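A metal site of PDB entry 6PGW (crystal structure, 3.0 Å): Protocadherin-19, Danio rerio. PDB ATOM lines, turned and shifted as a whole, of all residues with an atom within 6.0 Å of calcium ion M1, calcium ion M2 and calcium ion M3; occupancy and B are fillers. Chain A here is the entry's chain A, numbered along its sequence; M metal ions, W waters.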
ATOM      1  N   GLU A 126      16.087 -12.959 -10.269  1.00  0.00           N
ATOM      2  CA  GLU A 126      15.279 -12.720  -9.059  1.00  0.00           C
ATOM      3  C   GLU A 126      16.110 -12.271  -7.904  1.00  0.00           C
ATOM      4  O   GLU A 126      17.224 -12.767  -7.707  1.00  0.00           O
ATOM      5  CB  GLU A 126      14.645 -13.990  -8.552  1.00  0.00           C
ATOM      6  CG  GLU A 126      13.855 -14.800  -9.524  1.00  0.00           C
ATOM      7  CD  GLU A 126      13.242 -15.961  -8.839  1.00  0.00           C
ATOM      8  OE1 GLU A 126      13.755 -17.069  -8.974  1.00  0.00           O
ATOM      9  OE2 GLU A 126      12.313 -15.721  -8.074  1.00  0.00           O
ATOM     10  N   ASN A 127      15.532 -11.428  -7.058  1.00  0.00           N
ATOM     11  CA  ASN A 127      16.196 -10.912  -5.866  1.00  0.00           C
ATOM     12  C   ASN A 127      17.689 -10.657  -6.108  1.00  0.00           C
ATOM     13  O   ASN A 127      18.537 -10.946  -5.256  1.00  0.00           O
ATOM     14  CB  ASN A 127      15.958 -11.854  -4.633  1.00  0.00           C
ATOM     15  CG  ASN A 127      16.377 -13.310  -4.883  1.00  0.00           C
ATOM     16  OD1 ASN A 127      17.486 -13.584  -5.340  1.00  0.00           O
ATOM     17  ND2 ASN A 127      15.486 -14.254  -4.580  1.00  0.00           N
ATOM     18  N   LEU A 177      13.088  -8.469  -5.931  1.00  0.00           N
ATOM     19  CA  LEU A 177      12.393  -9.078  -7.062  1.00  0.00           C
ATOM     20  C   LEU A 177      12.132 -10.530  -6.809  1.00  0.00           C
ATOM     21  O   LEU A 177      13.055 -11.298  -6.531  1.00  0.00           O
ATOM     22  CB  LEU A 177      13.185  -8.918  -8.357  1.00  0.00           C
ATOM     23  CG  LEU A 177      13.792  -7.547  -8.624  1.00  0.00           C
ATOM     24  CD1 LEU A 177      15.000  -7.680  -9.555  1.00  0.00           C
ATOM     25  CD2 LEU A 177      12.731  -6.598  -9.198  1.00  0.00           C
ATOM     26  N   ASP A 178      10.870 -10.918  -6.931  1.00  0.00           N
ATOM     27  CA  ASP A 178      10.458 -12.299  -6.839  1.00  0.00           C
ATOM     28  C   ASP A 178       9.775 -12.669  -8.142  1.00  0.00           C
ATOM     29  O   ASP A 178       8.788 -12.041  -8.520  1.00  0.00           O
ATOM     30  CB  ASP A 178       9.508 -12.470  -5.670  1.00  0.00           C
ATOM     31  CG  ASP A 178       9.294 -13.915  -5.296  1.00  0.00           C
ATOM     32  OD1 ASP A 178       9.914 -14.831  -5.893  1.00  0.00           O
ATOM     33  OD2 ASP A 178       8.492 -14.143  -4.372  1.00  0.00           O
ATOM     34  N   ARG A 179      10.327 -13.669  -8.857  1.00  0.00           N
ATOM     35  CA  ARG A 179       9.749 -14.161 -10.111  1.00  0.00           C
ATOM     36  C   ARG A 179       8.395 -14.831  -9.877  1.00  0.00           C
ATOM     37  O   ARG A 179       7.429 -14.616 -10.629  1.00  0.00           O
ATOM     38  CB  ARG A 179      10.697 -15.153 -10.788  1.00  0.00           C
ATOM     39  CG  ARG A 179      10.059 -15.931 -11.926  1.00  0.00           C
ATOM     40  CD  ARG A 179      11.030 -16.239 -13.026  1.00  0.00           C
ATOM     41  NE  ARG A 179      10.323 -16.681 -14.239  1.00  0.00           N
ATOM     42  CZ  ARG A 179      10.202 -15.967 -15.373  1.00  0.00           C
ATOM     43  NH1 ARG A 179       9.542 -16.497 -16.387  1.00  0.00           N
ATOM     44  NH2 ARG A 179      10.714 -14.732 -15.499  1.00  0.00           N
ATOM     45  N   GLU A 180       8.334 -15.631  -8.809  1.00  0.00           N
ATOM     46  CA  GLU A 180       7.115 -16.323  -8.425  1.00  0.00           C
ATOM     47  C   GLU A 180       5.959 -15.337  -8.232  1.00  0.00           C
ATOM     48  O   GLU A 180       4.813 -15.705  -8.428  1.00  0.00           O
ATOM     49  CB  GLU A 180       7.340 -17.165  -7.165  1.00  0.00           C
ATOM     50  CG  GLU A 180       8.076 -18.492  -7.431  1.00  0.00           C
ATOM     51  CD  GLU A 180       9.559 -18.314  -7.782  1.00  0.00           C
ATOM     52  OE1 GLU A 180      10.113 -19.100  -8.590  1.00  0.00           O
ATOM     53  OE2 GLU A 180      10.168 -17.378  -7.273  1.00  0.00           O
ATOM     54  N   ASP A 211      14.710 -16.489 -13.839  1.00  0.00           N
ATOM     55  CA  ASP A 211      14.411 -17.398 -12.732  1.00  0.00           C
ATOM     56  C   ASP A 211      15.665 -17.879 -12.033  1.00  0.00           C
ATOM     57  O   ASP A 211      16.695 -18.114 -12.653  1.00  0.00           O
ATOM     58  CB  ASP A 211      13.628 -18.618 -13.243  1.00  0.00           C
ATOM     59  CG  ASP A 211      13.096 -19.518 -12.090  1.00  0.00           C
ATOM     60  OD1 ASP A 211      12.528 -19.000 -11.051  1.00  0.00           O
ATOM     61  OD2 ASP A 211      13.264 -20.756 -12.238  1.00  0.00           O
ATOM     62  N   GLU A 212      15.541 -18.023 -10.730  1.00  0.00           N
ATOM     63  CA  GLU A 212      16.507 -18.674  -9.905  1.00  0.00           C
ATOM     64  C   GLU A 212      15.816 -19.856  -9.243  1.00  0.00           C
ATOM     65  O   GLU A 212      14.557 -19.882  -9.106  1.00  0.00           O
ATOM     66  CB  GLU A 212      17.027 -17.703  -8.835  1.00  0.00           C
ATOM     67  CG  GLU A 212      18.214 -16.868  -9.266  1.00  0.00           C
ATOM     68  CD  GLU A 212      19.359 -17.711  -9.803  1.00  0.00           C
ATOM     69  OE1 GLU A 212      20.111 -17.205 -10.663  1.00  0.00           O
ATOM     70  OE2 GLU A 212      19.494 -18.896  -9.389  1.00  0.00           O
ATOM     71  N   ASN A 213      16.626 -20.844  -8.891  1.00  0.00           N
ATOM     72  CA  ASN A 213      16.178 -22.013  -8.184  1.00  0.00           C
ATOM     73  C   ASN A 213      16.226 -21.612  -6.727  1.00  0.00           C
ATOM     74  O   ASN A 213      17.136 -21.958  -6.024  1.00  0.00           O
ATOM     75  CB  ASN A 213      17.168 -23.159  -8.465  1.00  0.00           C
ATOM     76  CG  ASN A 213      16.619 -24.517  -8.069  1.00  0.00           C
ATOM     77  OD1 ASN A 213      15.417 -24.776  -8.119  1.00  0.00           O
ATOM     78  ND2 ASN A 213      17.525 -25.427  -7.690  1.00  0.00           N
ATOM     79  N   ASP A 214      15.303 -20.775  -6.294  1.00  0.00           N
ATOM     80  CA  ASP A 214      15.355 -20.258  -4.922  1.00  0.00           C
ATOM     81  C   ASP A 214      14.371 -20.942  -3.996  1.00  0.00           C
ATOM     82  O   ASP A 214      14.410 -20.703  -2.783  1.00  0.00           O
ATOM     83  CB  ASP A 214      15.243 -18.720  -4.856  1.00  0.00           C
ATOM     84  CG  ASP A 214      14.159 -18.150  -5.745  1.00  0.00           C
ATOM     85  OD1 ASP A 214      13.646 -18.842  -6.678  1.00  0.00           O
ATOM     86  OD2 ASP A 214      13.874 -16.986  -5.512  1.00  0.00           O
ATOM     87  N   ASN A 215      13.530 -21.829  -4.539  1.00  0.00           N
ATOM     88  CA  ASN A 215      12.551 -22.610  -3.755  1.00  0.00           C
ATOM     89  C   ASN A 215      12.666 -24.055  -4.125  1.00  0.00           C
ATOM     90  O   ASN A 215      12.916 -24.346  -5.272  1.00  0.00           O
ATOM     91  CB  ASN A 215      11.160 -22.205  -4.128  1.00  0.00           C
ATOM     92  CG  ASN A 215      10.919 -20.745  -3.956  1.00  0.00           C
ATOM     93  OD1 ASN A 215       9.957 -20.224  -4.482  1.00  0.00           O
ATOM     94  ND2 ASN A 215      11.778 -20.077  -3.206  1.00  0.00           N
ATOM     95  N   PRO A 216      12.404 -24.977  -3.172  1.00  0.00           N
ATOM     96  CA  PRO A 216      12.324 -26.398  -3.496  1.00  0.00           C
ATOM     97  C   PRO A 216      10.864 -26.868  -3.748  1.00  0.00           C
ATOM     98  O   PRO A 216       9.919 -26.048  -3.633  1.00  0.00           O
ATOM     99  CB  PRO A 216      12.876 -27.048  -2.227  1.00  0.00           C
ATOM    100  CG  PRO A 216      12.339 -26.179  -1.141  1.00  0.00           C
ATOM    101  CD  PRO A 216      12.231 -24.773  -1.718  1.00  0.00           C
ATOM    102  N   PRO A 217      10.679 -28.174  -4.056  1.00  0.00           N
ATOM    103  CA  PRO A 217       9.317 -28.714  -4.171  1.00  0.00           C
ATOM    104  C   PRO A 217       8.673 -28.828  -2.808  1.00  0.00           C
ATOM    105  O   PRO A 217       9.221 -29.461  -1.903  1.00  0.00           O
ATOM    106  CB  PRO A 217       9.511 -30.099  -4.811  1.00  0.00           C
ATOM    107  CG  PRO A 217      10.945 -30.177  -5.218  1.00  0.00           C
ATOM    108  CD  PRO A 217      11.696 -29.211  -4.351  1.00  0.00           C
ATOM    109  N   ASP A 245       7.006 -27.475  -7.260  1.00  0.00           N
ATOM    110  CA  ASP A 245       8.067 -26.524  -7.180  1.00  0.00           C
ATOM    111  C   ASP A 245       7.715 -25.329  -8.052  1.00  0.00           C
ATOM    112  O   ASP A 245       7.410 -25.480  -9.247  1.00  0.00           O
ATOM    113  CB  ASP A 245       9.346 -27.161  -7.640  1.00  0.00           C
ATOM    114  CG  ASP A 245      10.533 -26.272  -7.443  1.00  0.00           C
ATOM    115  OD1 ASP A 245      10.500 -25.116  -7.936  1.00  0.00           O
ATOM    116  OD2 ASP A 245      11.509 -26.731  -6.843  1.00  0.00           O
ATOM    117  N   PRO A 246       7.770 -24.127  -7.473  1.00  0.00           N
ATOM    118  CA  PRO A 246       7.316 -22.946  -8.213  1.00  0.00           C
ATOM    119  C   PRO A 246       8.289 -22.394  -9.251  1.00  0.00           C
ATOM    120  O   PRO A 246       7.916 -21.537 -10.015  1.00  0.00           O
ATOM    121  CB  PRO A 246       7.060 -21.918  -7.118  1.00  0.00           C
ATOM    122  CG  PRO A 246       7.930 -22.335  -5.993  1.00  0.00           C
ATOM    123  CD  PRO A 246       8.136 -23.808  -6.088  1.00  0.00           C
ATOM    124  N   ASP A 247       9.524 -22.903  -9.289  1.00  0.00           N
ATOM    125  CA  ASP A 247      10.500 -22.415 -10.245  1.00  0.00           C
ATOM    126  C   ASP A 247      10.251 -22.844 -11.666  1.00  0.00           C
ATOM    127  O   ASP A 247       9.378 -23.671 -11.953  1.00  0.00           O
ATOM    128  CB  ASP A 247      11.871 -22.898  -9.867  1.00  0.00           C
ATOM    129  CG  ASP A 247      12.276 -22.436  -8.561  1.00  0.00           C
ATOM    130  OD1 ASP A 247      12.115 -21.217  -8.305  1.00  0.00           O
ATOM    131  OD2 ASP A 247      12.717 -23.256  -7.761  1.00  0.00           O
ATOM    132  N   LEU A 248      11.062 -22.277 -12.542  1.00  0.00           N
ATOM    133  CA  LEU A 248      10.965 -22.523 -13.963  1.00  0.00           C
ATOM    134  C   LEU A 248      11.742 -23.732 -14.384  1.00  0.00           C
ATOM    135  O   LEU A 248      12.906 -23.903 -14.030  1.00  0.00           O
ATOM    136  CB  LEU A 248      11.444 -21.317 -14.749  1.00  0.00           C
ATOM    137  CG  LEU A 248      10.316 -20.503 -15.337  1.00  0.00           C
ATOM    138  CD1 LEU A 248       9.383 -19.960 -14.260  1.00  0.00           C
ATOM    139  CD2 LEU A 248      10.912 -19.375 -16.191  1.00  0.00           C
ATOM    140  N   MET A 250      13.633 -27.001 -15.082  1.00  0.00           N
ATOM    141  CA  MET A 250      14.443 -27.951 -14.384  1.00  0.00           C
ATOM    142  C   MET A 250      14.469 -27.584 -12.947  1.00  0.00           C
ATOM    143  O   MET A 250      14.510 -28.451 -12.076  1.00  0.00           O
ATOM    144  CB  MET A 250      15.841 -27.829 -14.870  1.00  0.00           C
ATOM    145  CG  MET A 250      15.974 -28.007 -16.363  1.00  0.00           C
ATOM    146  SD  MET A 250      16.683 -29.601 -16.732  1.00  0.00           S
ATOM    147  CE  MET A 250      18.400 -29.336 -16.263  1.00  0.00           C
ATOM    148  N   ASN A 251      14.534 -26.292 -12.679  1.00  0.00           N
ATOM    149  CA  ASN A 251      14.588 -25.821 -11.311  1.00  0.00           C
ATOM    150  C   ASN A 251      13.353 -26.245 -10.563  1.00  0.00           C
ATOM    151  O   ASN A 251      13.365 -26.410  -9.338  1.00  0.00           O
ATOM    152  CB  ASN A 251      14.767 -24.294 -11.260  1.00  0.00           C
ATOM    153  CG  ASN A 251      16.216 -23.842 -11.483  1.00  0.00           C
ATOM    154  OD1 ASN A 251      16.493 -22.650 -11.525  1.00  0.00           O
ATOM    155  ND2 ASN A 251      17.146 -24.798 -11.588  1.00  0.00           N
ATOM    156  N   GLY A 252      12.268 -26.416 -11.316  1.00  0.00           N
ATOM    157  CA  GLY A 252      10.968 -26.744 -10.776  1.00  0.00           C
ATOM    158  C   GLY A 252      10.347 -28.096 -11.142  1.00  0.00           C
ATOM    159  O   GLY A 252       9.179 -28.333 -10.880  1.00  0.00           O
ATOM    160  N   ASP A 302      14.891 -31.404  -7.570  1.00  0.00           N
ATOM    161  CA  ASP A 302      14.678 -30.654  -8.816  1.00  0.00           C
ATOM    162  C   ASP A 302      15.991 -30.371  -9.487  1.00  0.00           C
ATOM    163  O   ASP A 302      17.012 -30.308  -8.822  1.00  0.00           O
ATOM    164  CB  ASP A 302      14.040 -29.326  -8.496  1.00  0.00           C
ATOM    165  CG  ASP A 302      14.855 -28.526  -7.508  1.00  0.00           C
ATOM    166  OD1 ASP A 302      15.812 -29.064  -6.918  1.00  0.00           O
ATOM    167  OD2 ASP A 302      14.545 -27.385  -7.303  1.00  0.00           O
ATOM    168  N   LEU A 308      17.797 -28.901  -5.160  1.00  0.00           N
ATOM    169  CA  LEU A 308      17.238 -28.779  -3.816  1.00  0.00           C
ATOM    170  C   LEU A 308      16.249 -29.896  -3.463  1.00  0.00           C
ATOM    171  O   LEU A 308      15.660 -30.507  -4.348  1.00  0.00           O
ATOM    172  CB  LEU A 308      16.564 -27.421  -3.671  1.00  0.00           C
ATOM    173  CG  LEU A 308      17.556 -26.271  -3.763  1.00  0.00           C
ATOM    174  CD1 LEU A 308      16.782 -24.984  -3.744  1.00  0.00           C
ATOM    175  CD2 LEU A 308      18.587 -26.332  -2.642  1.00  0.00           C
HETATM  176 CA    CA M   1      13.368 -25.419  -7.257  1.00  0.00          CA
HETATM  177 CA    CA M   2      12.445 -18.945  -8.696  1.00  0.00          CA
HETATM  178 CA    CA M   3      11.717 -16.323  -5.937  1.00  0.00          CA
HETATM  179  O   HOH W   1      12.836 -15.305  -4.170  1.00  0.00           O
HETATM  180  O   HOH W   2      10.360 -16.805  -4.126  1.00  0.00           O
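Calcium ion M1 is bound by OD2 of Asp 302 (2.3 Å), O of Asn 215 (2.3 Å), O of Asn 251 (2.3 Å), OD2 of Asp 245 (2.3 Å), OD2 of Asp 247 (2.3 Å) and OD1 of Asn 213 (2.3 Å).
Calcium ion M1 has six donor atoms within binding distance.
Slightly farther from calcium ion M1 lies OD1 of Asp 245 (3.0 Å).
Six residues have an atom within 4 Å of calcium ion M1: Asn 213, Asn 215, Asp 245, Asp 247, Asn 251 and Asp 302.
The side-chain carboxylate (OD2) of Asp 211 lies within hydrogen-bond range of the backbone NH (N) of Leu 248, 2.7 Å away.
The side-chain carboxylate (OD2) of Asp 214 lies close to the side-chain amide nitrogen (ND2) of Asn 127, 3.3 Å away.
N of Arg 179 lies close to OE2 of Glu 126 (3.0 Å).
OD1 of Asp 302 is in hydrogen-bond range of N of Leu 308, at 2.7 Å.
Within 4 Å of calcium ion M3: Glu 126, Asp 178, Glu 180 and Asp 214.
The nearest printed residue that does not touch calcium ion M3 is Arg 179 (4.2 Å).
Six residues have an atom within 4 Å of calcium ion M2: Glu 126, Glu 180, Asp 211, Glu 212, Asp 214 and Asp 247.
The nearest printed residue that does not touch calcium ion M2 is Asn 213 (4.6 Å).
Calcium ion M2 is bound by OE1 of Glu 126 (2.3 Å).
OD1 of Asp 247 binds calcium ion M2, at 2.3 Å.
OE1 of Glu 180 binds calcium ion M2 (2.3 Å).
The backbone carbonyl oxygen (O) of Glu 212 is bound to calcium ion M2 (2.3 Å).
Calcium ion M2 is bound by OD1 of Asp 214, at 2.4 Å.
OD1 of Asp 211 is bound to calcium ion M2 (2.4 Å).
Slightly farther from calcium ion M2 lies the side-chain carboxylate (OE2) of Glu 180 (3.1 Å).
Calcium ion M3 is bound by OD2 of Asp 214 (2.3 Å), OE2 of Glu 126 (2.3 Å), OE2 of Glu 180 (2.3 Å), water W2 (2.3 Å), water W1 (2.3 Å) and OD1 of Asp 178 (2.3 Å).
Calcium ion M3 has six donor atoms within binding distance.
Water W2 lies within hydrogen-bond range of the side-chain carboxylate (OD2) of Asp 178 (3.3 Å) and the side-chain amide oxygen (OD1) of Asn 215 (3.5 Å).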
